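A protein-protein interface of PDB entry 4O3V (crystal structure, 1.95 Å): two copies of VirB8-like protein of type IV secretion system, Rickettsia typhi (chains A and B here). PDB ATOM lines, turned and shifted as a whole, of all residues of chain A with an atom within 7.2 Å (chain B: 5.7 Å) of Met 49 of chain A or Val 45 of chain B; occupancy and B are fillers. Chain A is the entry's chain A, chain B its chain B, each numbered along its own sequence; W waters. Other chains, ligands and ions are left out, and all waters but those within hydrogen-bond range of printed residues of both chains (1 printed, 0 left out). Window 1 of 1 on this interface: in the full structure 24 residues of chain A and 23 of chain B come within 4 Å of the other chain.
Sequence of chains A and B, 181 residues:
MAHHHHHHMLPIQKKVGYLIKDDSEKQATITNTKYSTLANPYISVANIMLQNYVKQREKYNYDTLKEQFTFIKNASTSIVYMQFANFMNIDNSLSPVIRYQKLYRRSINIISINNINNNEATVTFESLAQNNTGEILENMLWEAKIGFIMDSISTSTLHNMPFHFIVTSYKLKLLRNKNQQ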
ATOM      1  N   ILE A  43      -9.490  16.831  15.673  1.00  0.00           N
ATOM      2  CA  ILE A  43     -10.929  16.588  15.769  1.00  0.00           C
ATOM      3  C   ILE A  43     -11.575  16.465  14.373  1.00  0.00           C
ATOM      4  O   ILE A  43     -12.452  15.600  14.170  1.00  0.00           O
ATOM      5  CB  ILE A  43     -11.635  17.661  16.638  1.00  0.00           C
ATOM      6  CG1 ILE A  43     -11.261  17.492  18.118  1.00  0.00           C
ATOM      7  CG2 ILE A  43     -13.149  17.601  16.477  1.00  0.00           C
ATOM      8  CD1 ILE A  43     -11.621  16.152  18.748  1.00  0.00           C
ATOM      9  N   SER A  44     -11.157  17.270  13.387  1.00  0.00           N
ATOM     10  CA  SER A  44     -11.737  17.154  12.050  1.00  0.00           C
ATOM     11  C   SER A  44     -11.474  15.746  11.468  1.00  0.00           C
ATOM     12  O   SER A  44     -12.340  15.136  10.805  1.00  0.00           O
ATOM     13  CB  SER A  44     -11.209  18.263  11.126  1.00  0.00           C
ATOM     14  OG  SER A  44      -9.783  18.268  11.081  1.00  0.00           O
ATOM     15  N   VAL A  45     -10.287  15.217  11.749  1.00  0.00           N
ATOM     16  CA  VAL A  45      -9.888  13.897  11.262  1.00  0.00           C
ATOM     17  C   VAL A  45     -10.657  12.844  12.029  1.00  0.00           C
ATOM     18  O   VAL A  45     -11.194  11.921  11.410  1.00  0.00           O
ATOM     19  CB  VAL A  45      -8.361  13.655  11.344  1.00  0.00           C
ATOM     20  CG1 VAL A  45      -8.009  12.211  10.986  1.00  0.00           C
ATOM     21  CG2 VAL A  45      -7.648  14.576  10.386  1.00  0.00           C
ATOM     22  N   ALA A  46     -10.740  12.961  13.348  1.00  0.00           N
ATOM     23  CA  ALA A  46     -11.499  11.981  14.136  1.00  0.00           C
ATOM     24  C   ALA A  46     -12.939  11.912  13.657  1.00  0.00           C
ATOM     25  O   ALA A  46     -13.501  10.827  13.595  1.00  0.00           O
ATOM     26  CB  ALA A  46     -11.486  12.305  15.626  1.00  0.00           C
ATOM     27  N   ASN A  47     -13.525  13.056  13.311  1.00  0.00           N
ATOM     28  CA  ASN A  47     -14.918  13.050  12.866  1.00  0.00           C
ATOM     29  C   ASN A  47     -15.144  12.321  11.541  1.00  0.00           C
ATOM     30  O   ASN A  47     -16.151  11.630  11.396  1.00  0.00           O
ATOM     31  CB  ASN A  47     -15.530  14.435  12.825  1.00  0.00           C
ATOM     32  CG  ASN A  47     -15.767  15.001  14.222  1.00  0.00           C
ATOM     33  OD1 ASN A  47     -15.753  14.287  15.199  1.00  0.00           O
ATOM     34  ND2 ASN A  47     -15.978  16.276  14.300  1.00  0.00           N
ATOM     35  N   ILE A  48     -14.200  12.430  10.612  1.00  0.00           N
ATOM     36  CA  ILE A  48     -14.220  11.616   9.410  1.00  0.00           C
ATOM     37  C   ILE A  48     -14.181  10.116   9.737  1.00  0.00           C
ATOM     38  O   ILE A  48     -14.972   9.339   9.202  1.00  0.00           O
ATOM     39  CB  ILE A  48     -13.072  11.999   8.441  1.00  0.00           C
ATOM     40  CG1 ILE A  48     -13.365  13.393   7.931  1.00  0.00           C
ATOM     41  CG2 ILE A  48     -12.979  11.001   7.304  1.00  0.00           C
ATOM     42  CD1 ILE A  48     -12.211  14.024   7.242  1.00  0.00           C
ATOM     43  N   MET A  49     -13.279   9.725  10.633  1.00  0.00           N
ATOM     44  CA  MET A  49     -13.172   8.333  11.030  1.00  0.00           C
ATOM     45  C   MET A  49     -14.419   7.846  11.793  1.00  0.00           C
ATOM     46  O   MET A  49     -14.847   6.729  11.603  1.00  0.00           O
ATOM     47  CB  MET A  49     -11.948   8.128  11.941  1.00  0.00           C
ATOM     48  CG  MET A  49     -10.651   8.615  11.393  1.00  0.00           C
ATOM     49  SD  MET A  49     -10.345   7.732   9.880  1.00  0.00           S
ATOM     50  CE  MET A  49      -8.858   8.536   9.288  1.00  0.00           C
ATOM     51  N   LEU A  50     -14.949   8.670  12.697  1.00  0.00           N
ATOM     52  CA  LEU A  50     -16.162   8.354  13.448  1.00  0.00           C
ATOM     53  C   LEU A  50     -17.412   8.182  12.598  1.00  0.00           C
ATOM     54  O   LEU A  50     -18.156   7.200  12.785  1.00  0.00           O
ATOM     55  CB  LEU A  50     -16.431   9.379  14.550  1.00  0.00           C
ATOM     56  CG  LEU A  50     -15.435   9.372  15.719  1.00  0.00           C
ATOM     57  CD1 LEU A  50     -15.458  10.717  16.446  1.00  0.00           C
ATOM     58  CD2 LEU A  50     -15.754   8.244  16.683  1.00  0.00           C
ATOM     59  N   GLN A  51     -17.632   9.098  11.667  1.00  0.00           N
ATOM     60  CA  GLN A  51     -18.752   8.954  10.734  1.00  0.00           C
ATOM     61  C   GLN A  51     -18.632   7.686   9.916  1.00  0.00           C
ATOM     62  O   GLN A  51     -19.611   6.945   9.774  1.00  0.00           O
ATOM     63  CB  GLN A  51     -18.828  10.137   9.792  1.00  0.00           C
ATOM     64  CG  GLN A  51     -19.281  11.369  10.519  1.00  0.00           C
ATOM     65  CD  GLN A  51     -19.572  12.484   9.555  1.00  0.00           C
ATOM     66  OE1 GLN A  51     -20.617  12.497   8.898  1.00  0.00           O
ATOM     67  NE2 GLN A  51     -18.618  13.374   9.410  1.00  0.00           N
ATOM     68  N   ASN A  52     -17.441   7.444   9.374  1.00  0.00           N
ATOM     69  CA  ASN A  52     -17.205   6.227   8.613  1.00  0.00           C
ATOM     70  C   ASN A  52     -17.457   4.957   9.447  1.00  0.00           C
ATOM     71  O   ASN A  52     -18.111   3.993   8.983  1.00  0.00           O
ATOM     72  CB  ASN A  52     -15.813   6.212   8.043  1.00  0.00           C
ATOM     73  CG  ASN A  52     -15.623   5.079   7.068  1.00  0.00           C
ATOM     74  OD1 ASN A  52     -16.244   5.051   6.011  1.00  0.00           O
ATOM     75  ND2 ASN A  52     -14.722   4.170   7.384  1.00  0.00           N
ATOM     76  N   TYR A  53     -16.976   4.951  10.686  1.00  0.00           N
ATOM     77  CA  TYR A  53     -17.142   3.779  11.551  1.00  0.00           C
ATOM     78  C   TYR A  53     -18.619   3.507  11.809  1.00  0.00           C
ATOM     79  O   TYR A  53     -19.067   2.351  11.672  1.00  0.00           O
ATOM     80  CB  TYR A  53     -16.391   3.955  12.881  1.00  0.00           C
ATOM     81  CG  TYR A  53     -16.431   2.750  13.782  1.00  0.00           C
ATOM     82  CD1 TYR A  53     -17.470   2.559  14.661  1.00  0.00           C
ATOM     83  CD2 TYR A  53     -15.420   1.816  13.774  1.00  0.00           C
ATOM     84  CE1 TYR A  53     -17.508   1.475  15.499  1.00  0.00           C
ATOM     85  CE2 TYR A  53     -15.441   0.729  14.635  1.00  0.00           C
ATOM     86  CZ  TYR A  53     -16.499   0.534  15.462  1.00  0.00           C
ATOM     87  OH  TYR A  53     -16.523  -0.569  16.324  1.00  0.00           O
ATOM     88  N   VAL A  54     -19.384   4.542  12.132  1.00  0.00           N
ATOM     89  CA  VAL A  54     -20.817   4.362  12.397  1.00  0.00           C
ATOM     90  C   VAL A  54     -21.547   3.853  11.149  1.00  0.00           C
ATOM     91  O   VAL A  54     -22.387   2.976  11.251  1.00  0.00           O
ATOM     92  CB  VAL A  54     -21.477   5.670  12.953  1.00  0.00           C
ATOM     93  CG1 VAL A  54     -22.999   5.543  13.027  1.00  0.00           C
ATOM     94  CG2 VAL A  54     -20.944   5.951  14.337  1.00  0.00           C
ATOM     95  N   LYS A  55     -21.262   4.452   9.980  1.00  0.00           N
ATOM     96  CA  LYS A  55     -21.863   4.025   8.727  1.00  0.00           C
ATOM     97  C   LYS A  55     -21.554   2.553   8.439  1.00  0.00           C
ATOM     98  O   LYS A  55     -22.468   1.825   8.082  1.00  0.00           O
ATOM     99  CB  LYS A  55     -21.376   4.882   7.571  1.00  0.00           C
ATOM    100  CG  LYS A  55     -22.065   6.224   7.555  1.00  0.00           C
ATOM    101  CD  LYS A  55     -21.361   7.214   6.659  1.00  0.00           C
ATOM    102  CE  LYS A  55     -21.676   6.978   5.207  1.00  0.00           C
ATOM    103  NZ  LYS A  55     -23.120   7.265   4.924  1.00  0.00           N
ATOM    104  N   PHE A  71     -13.812  -4.934   8.781  1.00  0.00           N
ATOM    105  CA  PHE A  71     -13.653  -3.528   9.069  1.00  0.00           C
ATOM    106  C   PHE A  71     -13.739  -3.320  10.590  1.00  0.00           C
ATOM    107  O   PHE A  71     -12.880  -2.616  11.180  1.00  0.00           O
ATOM    108  CB  PHE A  71     -14.712  -2.676   8.355  1.00  0.00           C
ATOM    109  CG  PHE A  71     -14.716  -1.252   8.839  1.00  0.00           C
ATOM    110  CD1 PHE A  71     -13.829  -0.329   8.302  1.00  0.00           C
ATOM    111  CD2 PHE A  71     -15.566  -0.868   9.838  1.00  0.00           C
ATOM    112  CE1 PHE A  71     -13.768   0.972   8.806  1.00  0.00           C
ATOM    113  CE2 PHE A  71     -15.527   0.424  10.356  1.00  0.00           C
ATOM    114  CZ  PHE A  71     -14.642   1.351   9.807  1.00  0.00           C
ATOM    115  N   ILE A 113     -22.518  15.231  15.164  1.00  0.00           N
ATOM    116  CA  ILE A 113     -21.476  14.731  16.047  1.00  0.00           C
ATOM    117  C   ILE A 113     -21.217  15.739  17.135  1.00  0.00           C
ATOM    118  O   ILE A 113     -21.007  16.917  16.849  1.00  0.00           O
ATOM    119  CB  ILE A 113     -20.158  14.462  15.322  1.00  0.00           C
ATOM    120  CG1 ILE A 113     -20.394  13.467  14.196  1.00  0.00           C
ATOM    121  CG2 ILE A 113     -19.121  13.932  16.325  1.00  0.00           C
ATOM    122  CD1 ILE A 113     -19.149  12.891  13.564  1.00  0.00           C
ATOM    123  N   PHE A 148     -12.800   6.423  21.686  1.00  0.00           N
ATOM    124  CA  PHE A 148     -11.862   6.111  20.616  1.00  0.00           C
ATOM    125  C   PHE A 148     -10.488   6.622  21.003  1.00  0.00           C
ATOM    126  O   PHE A 148     -10.364   7.443  21.944  1.00  0.00           O
ATOM    127  CB  PHE A 148     -12.311   6.691  19.253  1.00  0.00           C
ATOM    128  CG  PHE A 148     -12.278   8.165  19.212  1.00  0.00           C
ATOM    129  CD1 PHE A 148     -13.345   8.905  19.725  1.00  0.00           C
ATOM    130  CD2 PHE A 148     -11.178   8.828  18.712  1.00  0.00           C
ATOM    131  CE1 PHE A 148     -13.291  10.277  19.743  1.00  0.00           C
ATOM    132  CE2 PHE A 148     -11.112  10.210  18.734  1.00  0.00           C
ATOM    133  CZ  PHE A 148     -12.179  10.930  19.228  1.00  0.00           C
ATOM    134  N   MET A 150      -6.736   7.637  18.722  1.00  0.00           N
ATOM    135  CA  MET A 150      -6.289   7.944  17.385  1.00  0.00           C
ATOM    136  C   MET A 150      -4.902   8.504  17.424  1.00  0.00           C
ATOM    137  O   MET A 150      -4.513   9.270  18.343  1.00  0.00           O
ATOM    138  CB  MET A 150      -7.245   8.959  16.714  1.00  0.00           C
ATOM    139  CG  MET A 150      -6.987   9.155  15.211  1.00  0.00           C
ATOM    140  SD  MET A 150      -8.222  10.238  14.415  1.00  0.00           S
ATOM    141  CE  MET A 150      -7.606  11.813  14.930  1.00  0.00           C
ATOM    142  N   PHE A 163      -1.875   5.225   9.684  1.00  0.00           N
ATOM    143  CA  PHE A 163      -2.505   6.145  10.584  1.00  0.00           C
ATOM    144  C   PHE A 163      -3.571   5.350  11.306  1.00  0.00           C
ATOM    145  O   PHE A 163      -4.481   4.808  10.688  1.00  0.00           O
ATOM    146  CB  PHE A 163      -3.099   7.374   9.839  1.00  0.00           C
ATOM    147  CG  PHE A 163      -3.639   8.402  10.746  1.00  0.00           C
ATOM    148  CD1 PHE A 163      -2.814   9.367  11.263  1.00  0.00           C
ATOM    149  CD2 PHE A 163      -4.965   8.386  11.125  1.00  0.00           C
ATOM    150  CE1 PHE A 163      -3.296  10.294  12.158  1.00  0.00           C
ATOM    151  CE2 PHE A 163      -5.449   9.329  12.016  1.00  0.00           C
ATOM    152  CZ  PHE A 163      -4.613  10.263  12.541  1.00  0.00           C
ATOM    153  N   HIS A 164      -3.467   5.261  12.627  1.00  0.00           N
ATOM    154  CA  HIS A 164      -4.355   4.365  13.365  1.00  0.00           C
ATOM    155  C   HIS A 164      -5.481   5.063  14.049  1.00  0.00           C
ATOM    156  O   HIS A 164      -5.285   6.133  14.624  1.00  0.00           O
ATOM    157  CB  HIS A 164      -3.539   3.570  14.397  1.00  0.00           C
ATOM    158  CG  HIS A 164      -2.430   2.780  13.794  1.00  0.00           C
ATOM    159  ND1 HIS A 164      -1.141   3.242  13.726  1.00  0.00           N
ATOM    160  CD2 HIS A 164      -2.407   1.532  13.272  1.00  0.00           C
ATOM    161  CE1 HIS A 164      -0.377   2.334  13.144  1.00  0.00           C
ATOM    162  NE2 HIS A 164      -1.125   1.297  12.855  1.00  0.00           N
ATOM    163  N   PHE A 165      -6.655   4.436  14.024  1.00  0.00           N
ATOM    164  CA  PHE A 165      -7.875   4.889  14.663  1.00  0.00           C
ATOM    165  C   PHE A 165      -8.560   3.632  15.194  1.00  0.00           C
ATOM    166  O   PHE A 165      -8.737   2.668  14.429  1.00  0.00           O
ATOM    167  CB  PHE A 165      -8.807   5.605  13.659  1.00  0.00           C
ATOM    168  CG  PHE A 165     -10.156   5.848  14.191  1.00  0.00           C
ATOM    169  CD1 PHE A 165     -10.431   6.988  14.931  1.00  0.00           C
ATOM    170  CD2 PHE A 165     -11.175   4.981  13.912  1.00  0.00           C
ATOM    171  CE1 PHE A 165     -11.708   7.224  15.419  1.00  0.00           C
ATOM    172  CE2 PHE A 165     -12.443   5.213  14.404  1.00  0.00           C
ATOM    173  CZ  PHE A 165     -12.698   6.328  15.183  1.00  0.00           C
ATOM    174  N   ILE A 166      -8.870   3.610  16.501  1.00  0.00           N
ATOM    175  CA  ILE A 166      -9.462   2.417  17.146  1.00  0.00           C
ATOM    176  C   ILE A 166     -10.603   2.851  18.047  1.00  0.00           C
ATOM    177  O   ILE A 166     -10.445   3.757  18.893  1.00  0.00           O
ATOM    178  CB  ILE A 166      -8.404   1.658  17.974  1.00  0.00           C
ATOM    179  CG1 ILE A 166      -7.268   1.144  17.095  1.00  0.00           C
ATOM    180  CG2 ILE A 166      -9.045   0.524  18.756  1.00  0.00           C
ATOM    181  CD1 ILE A 166      -7.660  -0.015  16.185  1.00  0.00           C
ATOM    182  N   VAL A 167     -11.756   2.216  17.888  1.00  0.00           N
ATOM    183  CA  VAL A 167     -12.892   2.424  18.771  1.00  0.00           C
ATOM    184  C   VAL A 167     -12.728   1.549  20.040  1.00  0.00           C
ATOM    185  O   VAL A 167     -12.532   0.314  19.969  1.00  0.00           O
ATOM    186  CB  VAL A 167     -14.229   2.139  18.053  1.00  0.00           C
ATOM    187  CG1 VAL A 167     -15.402   2.113  19.015  1.00  0.00           C
ATOM    188  CG2 VAL A 167     -14.443   3.193  16.966  1.00  0.00           C
ATOM    189  N   PRO B  41      -2.350  11.589   8.401  1.00  0.00           N
ATOM    190  CA  PRO B  41      -3.629  10.971   8.072  1.00  0.00           C
ATOM    191  C   PRO B  41      -4.082  11.131   6.635  1.00  0.00           C
ATOM    192  O   PRO B  41      -5.184  10.701   6.289  1.00  0.00           O
ATOM    193  CB  PRO B  41      -4.596  11.718   8.961  1.00  0.00           C
ATOM    194  CG  PRO B  41      -3.996  13.096   9.059  1.00  0.00           C
ATOM    195  CD  PRO B  41      -2.517  12.885   9.076  1.00  0.00           C
ATOM    196  N   TYR B  42      -3.271  11.764   5.796  1.00  0.00           N
ATOM    197  CA  TYR B  42      -3.703  12.107   4.449  1.00  0.00           C
ATOM    198  C   TYR B  42      -4.253  10.933   3.673  1.00  0.00           C
ATOM    199  O   TYR B  42      -5.370  11.001   3.173  1.00  0.00           O
ATOM    200  CB  TYR B  42      -2.536  12.770   3.671  1.00  0.00           C
ATOM    201  CG  TYR B  42      -2.852  13.155   2.254  1.00  0.00           C
ATOM    202  CD1 TYR B  42      -2.682  12.253   1.201  1.00  0.00           C
ATOM    203  CD2 TYR B  42      -3.254  14.436   1.947  1.00  0.00           C
ATOM    204  CE1 TYR B  42      -2.918  12.622  -0.116  1.00  0.00           C
ATOM    205  CE2 TYR B  42      -3.501  14.815   0.636  1.00  0.00           C
ATOM    206  CZ  TYR B  42      -3.346  13.911  -0.382  1.00  0.00           C
ATOM    207  OH  TYR B  42      -3.605  14.310  -1.666  1.00  0.00           O
ATOM    208  N   ILE B  43      -3.516   9.831   3.592  1.00  0.00           N
ATOM    209  CA  ILE B  43      -3.954   8.696   2.776  1.00  0.00           C
ATOM    210  C   ILE B  43      -5.175   8.024   3.406  1.00  0.00           C
ATOM    211  O   ILE B  43      -6.130   7.670   2.694  1.00  0.00           O
ATOM    212  CB  ILE B  43      -2.816   7.671   2.481  1.00  0.00           C
ATOM    213  CG1 ILE B  43      -1.751   8.279   1.528  1.00  0.00           C
ATOM    214  CG2 ILE B  43      -3.360   6.352   1.931  1.00  0.00           C
ATOM    215  CD1 ILE B  43      -2.208   8.526   0.102  1.00  0.00           C
ATOM    216  N   SER B  44      -5.168   7.866   4.728  1.00  0.00           N
ATOM    217  CA  SER B  44      -6.314   7.244   5.404  1.00  0.00           C
ATOM    218  C   SER B  44      -7.607   8.054   5.177  1.00  0.00           C
ATOM    219  O   SER B  44      -8.663   7.476   4.897  1.00  0.00           O
ATOM    220  CB  SER B  44      -6.049   7.068   6.877  1.00  0.00           C
ATOM    221  OG  SER B  44      -4.921   6.258   7.087  1.00  0.00           O
ATOM    222  N   VAL B  45      -7.524   9.376   5.237  1.00  0.00           N
ATOM    223  CA  VAL B  45      -8.681  10.218   4.964  1.00  0.00           C
ATOM    224  C   VAL B  45      -9.060  10.167   3.489  1.00  0.00           C
ATOM    225  O   VAL B  45     -10.241  10.047   3.142  1.00  0.00           O
ATOM    226  CB  VAL B  45      -8.414  11.656   5.439  1.00  0.00           C
ATOM    227  CG1 VAL B  45      -9.454  12.655   4.893  1.00  0.00           C
ATOM    228  CG2 VAL B  45      -8.356  11.718   6.947  1.00  0.00           C
ATOM    229  N   ALA B  46      -8.075  10.300   2.607  1.00  0.00           N
ATOM    230  CA  ALA B  46      -8.330  10.267   1.178  1.00  0.00           C
ATOM    231  C   ALA B  46      -9.030   8.977   0.804  1.00  0.00           C
ATOM    232  O   ALA B  46      -9.932   8.987  -0.038  1.00  0.00           O
ATOM    233  CB  ALA B  46      -7.037  10.405   0.385  1.00  0.00           C
ATOM    234  N   ASN B  47      -8.651   7.876   1.449  1.00  0.00           N
ATOM    235  CA  ASN B  47      -9.304   6.601   1.125  1.00  0.00           C
ATOM    236  C   ASN B  47     -10.781   6.580   1.443  1.00  0.00           C
ATOM    237  O   ASN B  47     -11.577   5.971   0.708  1.00  0.00           O
ATOM    238  CB  ASN B  47      -8.571   5.417   1.745  1.00  0.00           C
ATOM    239  CG  ASN B  47      -7.308   5.085   0.969  1.00  0.00           C
ATOM    240  OD1 ASN B  47      -7.125   5.566  -0.184  1.00  0.00           O
ATOM    241  ND2 ASN B  47      -6.448   4.298   1.552  1.00  0.00           N
ATOM    242  N   ILE B  48     -11.159   7.227   2.545  1.00  0.00           N
ATOM    243  CA  ILE B  48     -12.564   7.365   2.864  1.00  0.00           C
ATOM    244  C   ILE B  48     -13.282   8.250   1.823  1.00  0.00           C
ATOM    245  O   ILE B  48     -14.404   7.917   1.366  1.00  0.00           O
ATOM    246  CB  ILE B  48     -12.732   7.878   4.301  1.00  0.00           C
ATOM    247  CG1 ILE B  48     -12.306   6.754   5.269  1.00  0.00           C
ATOM    248  CG2 ILE B  48     -14.170   8.253   4.593  1.00  0.00           C
ATOM    249  CD1 ILE B  48     -12.132   7.244   6.684  1.00  0.00           C
ATOM    250  N   MET B  49     -12.622   9.336   1.413  1.00  0.00           N
ATOM    251  CA  MET B  49     -13.195  10.231   0.367  1.00  0.00           C
ATOM    252  C   MET B  49     -13.348   9.498  -0.973  1.00  0.00           C
ATOM    253  O   MET B  49     -14.361   9.626  -1.652  1.00  0.00           O
ATOM    254  CB  MET B  49     -12.336  11.486   0.178  1.00  0.00           C
ATOM    255  CG  MET B  49     -12.091  12.324   1.437  1.00  0.00           C
ATOM    256  SD  MET B  49     -13.647  12.892   2.099  1.00  0.00           S
ATOM    257  CE  MET B  49     -13.608  12.349   3.794  1.00  0.00           C
ATOM    258  N   LEU B  50     -12.347   8.715  -1.345  1.00  0.00           N
ATOM    259  CA  LEU B  50     -12.351   7.965  -2.611  1.00  0.00           C
ATOM    260  C   LEU B  50     -13.461   6.895  -2.629  1.00  0.00           C
ATOM    261  O   LEU B  50     -14.191   6.770  -3.621  1.00  0.00           O
ATOM    262  CB  LEU B  50     -10.988   7.259  -2.833  1.00  0.00           C
ATOM    263  CG  LEU B  50      -9.838   8.189  -3.213  1.00  0.00           C
ATOM    264  CD1 LEU B  50      -8.493   7.532  -2.941  1.00  0.00           C
ATOM    265  CD2 LEU B  50      -9.987   8.610  -4.663  1.00  0.00           C
ATOM    266  N   MET B 150      -6.133  16.761  -2.195  1.00  0.00           N
ATOM    267  CA  MET B 150      -6.757  17.158  -0.954  1.00  0.00           C
ATOM    268  C   MET B 150      -5.767  18.008  -0.209  1.00  0.00           C
ATOM    269  O   MET B 150      -4.564  17.946  -0.503  1.00  0.00           O
ATOM    270  CB  MET B 150      -7.075  15.876  -0.175  1.00  0.00           C
ATOM    271  CG  MET B 150      -7.922  16.060   1.044  1.00  0.00           C
ATOM    272  SD  MET B 150      -8.379  14.425   1.743  1.00  0.00           S
ATOM    273  CE  MET B 150      -6.824  13.913   2.446  1.00  0.00           C
ATOM    274  N   ILE B 153      -2.847  17.721   5.685  1.00  0.00           N
ATOM    275  CA  ILE B 153      -3.435  17.721   7.003  1.00  0.00           C
ATOM    276  C   ILE B 153      -2.280  17.672   7.958  1.00  0.00           C
ATOM    277  O   ILE B 153      -1.528  16.701   8.001  1.00  0.00           O
ATOM    278  CB  ILE B 153      -4.372  16.518   7.188  1.00  0.00           C
ATOM    279  CG1 ILE B 153      -5.389  16.478   6.033  1.00  0.00           C
ATOM    280  CG2 ILE B 153      -5.077  16.612   8.536  1.00  0.00           C
ATOM    281  CD1 ILE B 153      -6.233  15.216   5.965  1.00  0.00           C
ATOM    282  N   PHE B 163     -11.557  18.783   3.793  1.00  0.00           N
ATOM    283  CA  PHE B 163     -10.187  19.015   3.389  1.00  0.00           C
ATOM    284  C   PHE B 163     -10.046  19.376   1.888  1.00  0.00           C
ATOM    285  O   PHE B 163      -8.992  19.128   1.286  1.00  0.00           O
ATOM    286  CB  PHE B 163      -9.331  17.795   3.774  1.00  0.00           C
ATOM    287  CG  PHE B 163      -9.268  17.587   5.256  1.00  0.00           C
ATOM    288  CD1 PHE B 163      -8.571  18.466   6.045  1.00  0.00           C
ATOM    289  CD2 PHE B 163      -9.991  16.572   5.858  1.00  0.00           C
ATOM    290  CE1 PHE B 163      -8.526  18.305   7.431  1.00  0.00           C
ATOM    291  CE2 PHE B 163      -9.944  16.422   7.232  1.00  0.00           C
ATOM    292  CZ  PHE B 163      -9.222  17.274   8.003  1.00  0.00           C
HETATM  293  O   HOH W   1      -5.567   4.007   8.173  1.00  0.00           O
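Hydrophobic or aromatic side chains of chain A within 4 Å of the printed part of chain B: Val 45, Ile 48, Met 49 and Phe 163. Along chain B the printed residues that touch a printed residue of chain A span positions 41 to 163. Among the printed residues, no Asp or Glu carboxylate lies within 4 Å of a Lys or Arg side-chain nitrogen of the other chain.
Water W1 bridges the side-chain hydroxyl (OG) of Ser 44 of chain B (2.6 Å) and the backbone carbonyl oxygen (O) of Phe 163 of chain A (2.9 Å).
Ile 48 of chain A touches its own counterpart, Ile 48 of chain B. Ile 48 of chain A touches Met 49 of chain B, and with the chains exchanged Met 49 of chain A touches Ile 48 of chain B. Ile 48 of chain A touches Phe 163 of chain B, but with the chains exchanged Phe 163 of chain A does not touch Ile 48 of chain B (8.5 Å). Met 49 of chain A touches Ser 44 of chain B, but with the chains exchanged Ser 44 of chain A does not touch Met 49 of chain B (7.7 Å).
Of the printed residues of chain B, Met 49 of chain A touches Ser 44, Val 45 and Ile 48. Of the printed residues of chain A, Val 45 of chain B touches Ile 48 and Met 49. Printed residues of chain A within 4 Å of Met 49 of chain B: Ile 48. Of the printed residues of chain A, Phe 163 of chain B touches Ser 44 (3.3 Å), Val 45 (3.9 Å) and Ile 48 (3.3 Å). Of the printed residues of chain A, Ser 44 of chain B touches Met 49 and Phe 163. Of the printed residues of chain A, Ile 153 of chain B touches Val 45. Printed residues of chain B within 4 Å of Ser 44 of chain A: Phe 163. Val 54 of chain A touches none of the printed residues of chain B. Tyr 42 of chain B touches none of the printed residues of chain A. The nearest printed residue of chain B that does not touch Met 49 of chain A is Pro 41 of chain B (5.2 Å).
Among the printed residues, merely in contact across the chains: Ser 44 of chain A with Phe 163 of chain B, Ile 48 of chain A with Phe 163 of chain B, Phe 163 of chain A with Ser 44 of chain B, Phe 163 of chain A with Pro 41 of chain B, Met 49 of chain A with Ile 48 of chain B, Val 45 of chain A with Ile 153 of chain B, Ile 48 of chain A with Met 49 of chain B, Ile 48 of chain A with Val 45 of chain B, Ile 48 of chain A with Ile 48 of chain B, Val 45 of chain A with Phe 163 of chain B, Met 49 of chain A with Val 45 of chain B, Met 49 of chain A with Ser 44 of chain B and Val 45 of chain A with Pro 41 of chain B.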
